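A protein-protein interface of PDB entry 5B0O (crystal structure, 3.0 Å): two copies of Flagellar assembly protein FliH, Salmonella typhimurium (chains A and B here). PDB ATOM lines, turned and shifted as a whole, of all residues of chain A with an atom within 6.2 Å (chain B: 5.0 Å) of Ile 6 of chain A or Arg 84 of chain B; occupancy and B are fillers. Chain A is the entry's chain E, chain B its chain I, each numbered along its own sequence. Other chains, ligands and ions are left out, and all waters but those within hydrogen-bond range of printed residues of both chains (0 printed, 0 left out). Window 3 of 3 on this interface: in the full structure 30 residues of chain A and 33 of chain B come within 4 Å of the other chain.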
ATOM      1  N   PRO A   5      -4.022   3.944   4.038  1.00  0.00           N
ATOM      2  CA  PRO A   5      -4.834   2.816   4.507  1.00  0.00           C
ATOM      3  C   PRO A   5      -4.145   2.111   5.668  1.00  0.00           C
ATOM      4  O   PRO A   5      -4.485   2.348   6.829  1.00  0.00           O
ATOM      5  CB  PRO A   5      -4.891   1.902   3.283  1.00  0.00           C
ATOM      6  CG  PRO A   5      -3.622   2.179   2.550  1.00  0.00           C
ATOM      7  CD  PRO A   5      -3.260   3.616   2.819  1.00  0.00           C
ATOM      8  N   ILE A   6      -3.188   1.247   5.344  1.00  0.00           N
ATOM      9  CA  ILE A   6      -2.303   0.659   6.334  1.00  0.00           C
ATOM     10  C   ILE A   6      -1.675   1.786   7.144  1.00  0.00           C
ATOM     11  O   ILE A   6      -1.771   1.815   8.369  1.00  0.00           O
ATOM     12  CB  ILE A   6      -1.174  -0.131   5.650  1.00  0.00           C
ATOM     13  CG1 ILE A   6      -1.746  -1.079   4.592  1.00  0.00           C
ATOM     14  CG2 ILE A   6      -0.331  -0.872   6.678  1.00  0.00           C
ATOM     15  CD1 ILE A   6      -0.688  -1.714   3.718  1.00  0.00           C
ATOM     16  N   HIS A   7      -1.049   2.726   6.441  1.00  0.00           N
ATOM     17  CA  HIS A   7      -0.385   3.858   7.078  1.00  0.00           C
ATOM     18  C   HIS A   7      -1.379   4.712   7.865  1.00  0.00           C
ATOM     19  O   HIS A   7      -1.010   5.373   8.836  1.00  0.00           O
ATOM     20  CB  HIS A   7       0.335   4.715   6.032  1.00  0.00           C
ATOM     21  CG  HIS A   7       1.198   3.927   5.094  1.00  0.00           C
ATOM     22  ND1 HIS A   7       0.690   3.028   4.188  1.00  0.00           N
ATOM     23  CD2 HIS A   7       2.547   3.913   4.920  1.00  0.00           C
ATOM     24  CE1 HIS A   7       1.679   2.487   3.495  1.00  0.00           C
ATOM     25  NE2 HIS A   7       2.814   3.010   3.925  1.00  0.00           N
ATOM     26  N   ALA A   8      -2.637   4.702   7.437  1.00  0.00           N
ATOM     27  CA  ALA A   8      -3.672   5.479   8.112  1.00  0.00           C
ATOM     28  C   ALA A   8      -3.918   5.021   9.550  1.00  0.00           C
ATOM     29  O   ALA A   8      -3.739   5.793  10.491  1.00  0.00           O
ATOM     30  CB  ALA A   8      -4.965   5.446   7.313  1.00  0.00           C
ATOM     31  N   ARG A   9      -4.321   3.764   9.720  1.00  0.00           N
ATOM     32  CA  ARG A   9      -4.571   3.233  11.059  1.00  0.00           C
ATOM     33  C   ARG A   9      -3.436   2.413  11.661  1.00  0.00           C
ATOM     34  O   ARG A   9      -3.550   1.953  12.792  1.00  0.00           O
ATOM     35  CB  ARG A   9      -5.890   2.453  11.124  1.00  0.00           C
ATOM     36  CG  ARG A   9      -7.118   3.347  11.213  1.00  0.00           C
ATOM     37  CD  ARG A   9      -8.411   2.554  11.110  1.00  0.00           C
ATOM     38  NE  ARG A   9      -8.828   1.991  12.390  1.00  0.00           N
ATOM     39  CZ  ARG A   9      -9.401   2.697  13.359  1.00  0.00           C
ATOM     40  NH1 ARG A   9      -9.610   3.997  13.202  1.00  0.00           N
ATOM     41  NH2 ARG A   9      -9.758   2.108  14.490  1.00  0.00           N
ATOM     42  N   MET A  10      -2.351   2.212  10.922  1.00  0.00           N
ATOM     43  CA  MET A  10      -1.182   1.592  11.538  1.00  0.00           C
ATOM     44  C   MET A  10      -0.410   2.649  12.319  1.00  0.00           C
ATOM     45  O   MET A  10       0.386   2.326  13.200  1.00  0.00           O
ATOM     46  CB  MET A  10      -0.279   0.906  10.514  1.00  0.00           C
ATOM     47  CG  MET A  10       0.907   0.187  11.146  1.00  0.00           C
ATOM     48  SD  MET A  10       1.940  -0.679   9.950  1.00  0.00           S
ATOM     49  CE  MET A  10       0.887  -2.061   9.508  1.00  0.00           C
ATOM     50  N   GLN A  11      -0.636   3.913  11.972  1.00  0.00           N
ATOM     51  CA  GLN A  11      -0.133   5.025  12.773  1.00  0.00           C
ATOM     52  C   GLN A  11      -1.050   5.304  13.958  1.00  0.00           C
ATOM     53  O   GLN A  11      -0.614   5.809  14.994  1.00  0.00           O
ATOM     54  CB  GLN A  11       0.014   6.290  11.934  1.00  0.00           C
ATOM     55  CG  GLN A  11       0.324   7.519  12.769  1.00  0.00           C
ATOM     56  CD  GLN A  11       0.563   8.745  11.925  1.00  0.00           C
ATOM     57  OE1 GLN A  11       0.408   8.710  10.704  1.00  0.00           O
ATOM     58  NE2 GLN A  11       0.949   9.839  12.568  1.00  0.00           N
ATOM     59  N   LEU A  13      -2.386   3.149  15.943  1.00  0.00           N
ATOM     60  CA  LEU A  13      -1.849   2.362  17.050  1.00  0.00           C
ATOM     61  C   LEU A  13      -0.531   2.928  17.567  1.00  0.00           C
ATOM     62  O   LEU A  13      -0.277   2.919  18.773  1.00  0.00           O
ATOM     63  CB  LEU A  13      -1.672   0.893  16.651  1.00  0.00           C
ATOM     64  CG  LEU A  13      -2.938   0.049  16.462  1.00  0.00           C
ATOM     65  CD1 LEU A  13      -3.733   0.533  15.271  1.00  0.00           C
ATOM     66  CD2 LEU A  13      -2.582  -1.414  16.291  1.00  0.00           C
ATOM     67  N   ASP B  81      -6.531  -5.526  15.150  1.00  0.00           N
ATOM     68  CA  ASP B  81      -5.181  -5.050  14.841  1.00  0.00           C
ATOM     69  C   ASP B  81      -4.118  -5.913  15.517  1.00  0.00           C
ATOM     70  O   ASP B  81      -2.929  -5.607  15.466  1.00  0.00           O
ATOM     71  CB  ASP B  81      -5.008  -3.577  15.225  1.00  0.00           C
ATOM     72  CG  ASP B  81      -6.275  -2.968  15.783  1.00  0.00           C
ATOM     73  OD1 ASP B  81      -6.579  -1.806  15.441  1.00  0.00           O
ATOM     74  OD2 ASP B  81      -6.961  -3.647  16.572  1.00  0.00           O
ATOM     75  N   LEU B  82      -4.559  -6.987  16.161  1.00  0.00           N
ATOM     76  CA  LEU B  82      -3.652  -7.894  16.849  1.00  0.00           C
ATOM     77  C   LEU B  82      -2.547  -8.425  15.940  1.00  0.00           C
ATOM     78  O   LEU B  82      -1.363  -8.276  16.241  1.00  0.00           O
ATOM     79  CB  LEU B  82      -4.428  -9.061  17.459  1.00  0.00           C
ATOM     80  CG  LEU B  82      -3.549 -10.149  18.077  1.00  0.00           C
ATOM     81  CD1 LEU B  82      -2.599  -9.517  19.054  1.00  0.00           C
ATOM     82  CD2 LEU B  82      -4.376 -11.232  18.756  1.00  0.00           C
ATOM     83  N   GLN B  83      -2.934  -9.052  14.836  1.00  0.00           N
ATOM     84  CA  GLN B  83      -1.961  -9.629  13.919  1.00  0.00           C
ATOM     85  C   GLN B  83      -1.017  -8.548  13.388  1.00  0.00           C
ATOM     86  O   GLN B  83       0.187  -8.767  13.257  1.00  0.00           O
ATOM     87  CB  GLN B  83      -2.666 -10.346  12.762  1.00  0.00           C
ATOM     88  CG  GLN B  83      -1.720 -11.067  11.799  1.00  0.00           C
ATOM     89  CD  GLN B  83      -2.271 -11.161  10.384  1.00  0.00           C
ATOM     90  OE1 GLN B  83      -3.450 -10.903  10.143  1.00  0.00           O
ATOM     91  NE2 GLN B  83      -1.411 -11.526   9.439  1.00  0.00           N
ATOM     92  N   ARG B  84      -1.578  -7.381  13.090  1.00  0.00           N
ATOM     93  CA  ARG B  84      -0.824  -6.268  12.517  1.00  0.00           C
ATOM     94  C   ARG B  84       0.328  -5.817  13.418  1.00  0.00           C
ATOM     95  O   ARG B  84       1.450  -5.612  12.951  1.00  0.00           O
ATOM     96  CB  ARG B  84      -1.770  -5.097  12.238  1.00  0.00           C
ATOM     97  CG  ARG B  84      -1.122  -3.898  11.571  1.00  0.00           C
ATOM     98  CD  ARG B  84      -2.165  -2.836  11.238  1.00  0.00           C
ATOM     99  NE  ARG B  84      -3.333  -3.419  10.584  1.00  0.00           N
ATOM    100  CZ  ARG B  84      -3.489  -3.514   9.266  1.00  0.00           C
ATOM    101  NH1 ARG B  84      -2.553  -3.055   8.445  1.00  0.00           N
ATOM    102  NH2 ARG B  84      -4.586  -4.067   8.769  1.00  0.00           N
ATOM    103  N   VAL B  85       0.038  -5.664  14.707  1.00  0.00           N
ATOM    104  CA  VAL B  85       1.029  -5.245  15.695  1.00  0.00           C
ATOM    105  C   VAL B  85       2.158  -6.256  15.840  1.00  0.00           C
ATOM    106  O   VAL B  85       3.337  -5.910  15.755  1.00  0.00           O
ATOM    107  CB  VAL B  85       0.384  -5.075  17.084  1.00  0.00           C
ATOM    108  CG1 VAL B  85       1.439  -4.746  18.128  1.00  0.00           C
ATOM    109  CG2 VAL B  85      -0.694  -4.013  17.049  1.00  0.00           C
ATOM    110  N   GLU B  86       1.783  -7.509  16.069  1.00  0.00           N
ATOM    111  CA  GLU B  86       2.751  -8.565  16.328  1.00  0.00           C
ATOM    112  C   GLU B  86       3.712  -8.739  15.167  1.00  0.00           C
ATOM    113  O   GLU B  86       4.858  -9.129  15.357  1.00  0.00           O
ATOM    114  CB  GLU B  86       2.042  -9.885  16.619  1.00  0.00           C
ATOM    115  CG  GLU B  86       2.992 -11.010  16.973  1.00  0.00           C
ATOM    116  CD  GLU B  86       2.268 -12.293  17.304  1.00  0.00           C
ATOM    117  OE1 GLU B  86       1.049 -12.369  17.041  1.00  0.00           O
ATOM    118  OE2 GLU B  86       2.914 -13.224  17.828  1.00  0.00           O
ATOM    119  N   GLU B  87       3.236  -8.457  13.960  1.00  0.00           N
ATOM    120  CA  GLU B  87       4.101  -8.476  12.790  1.00  0.00           C
ATOM    121  C   GLU B  87       5.123  -7.344  12.876  1.00  0.00           C
ATOM    122  O   GLU B  87       6.294  -7.528  12.544  1.00  0.00           O
ATOM    123  CB  GLU B  87       3.275  -8.356  11.507  1.00  0.00           C
ATOM    124  CG  GLU B  87       2.320  -9.523  11.262  1.00  0.00           C
ATOM    125  CD  GLU B  87       1.408  -9.298  10.063  1.00  0.00           C
ATOM    126  OE1 GLU B  87       1.315  -8.146   9.587  1.00  0.00           O
ATOM    127  OE2 GLU B  87       0.784 -10.277   9.598  1.00  0.00           O
ATOM    128  N   MET B  88       4.669  -6.170  13.303  1.00  0.00           N
ATOM    129  CA  MET B  88       5.549  -5.014  13.467  1.00  0.00           C
ATOM    130  C   MET B  88       6.468  -5.086  14.691  1.00  0.00           C
ATOM    131  O   MET B  88       7.690  -4.988  14.570  1.00  0.00           O
ATOM    132  CB  MET B  88       4.712  -3.733  13.526  1.00  0.00           C
ATOM    133  CG  MET B  88       5.528  -2.455  13.623  1.00  0.00           C
ATOM    134  SD  MET B  88       6.610  -2.207  12.199  1.00  0.00           S
ATOM    135  CE  MET B  88       5.432  -2.274  10.847  1.00  0.00           C
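Of chain B, only Arg 84 (3.6 Å) comes within 4 Å of Ile 6 of chain A.
Printed residues of chain B within 4 Å of Met 10 of chain A: Arg 84 (3.4 Å) and Met 88 (3.9 Å).
Gln 11 of chain A touches none of the printed residues of chain B.
Arg 84 of chain B touches two residues of chain A.
Printed residues of chain A within 4 Å of Val 85 of chain B: Leu 13 (3.3 Å).
Of the printed residues of chain A, Met 88 of chain B touches Met 10 (3.9 Å).
The nearest printed residue of chain B that does not touch Ile 6 of chain A is Met 88 of chain B (7.2 Å).
The nearest printed residue of chain B that does not touch Met 10 of chain A is Glu 87 of chain B (6.1 Å).
No position is printed for both chains.
Of the 5 pairs that touch across the chains among the printed residues, none has its exchanged pair printed and touching as well.
Ile 6 of chain A touches Arg 84 of chain B (CG2 to NH1, 3.6 Å).
Arg 84 of chain B touches Met 10 of chain A (CG to CE, 3.4 Å).
Met 10 of chain A touches Met 88 of chain B (SD to CE, 3.9 Å).
Asp 81 of chain B touches Leu 13 of chain A.
Val 85 of chain B touches Leu 13 of chain A.
Hydrophobic or aromatic side chains of chain A within 4 Å of the printed part of chain B: Ile 6, Met 10 and Leu 13.
Along chain B the printed residues that touch a printed residue of chain A span positions 81 to 88.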
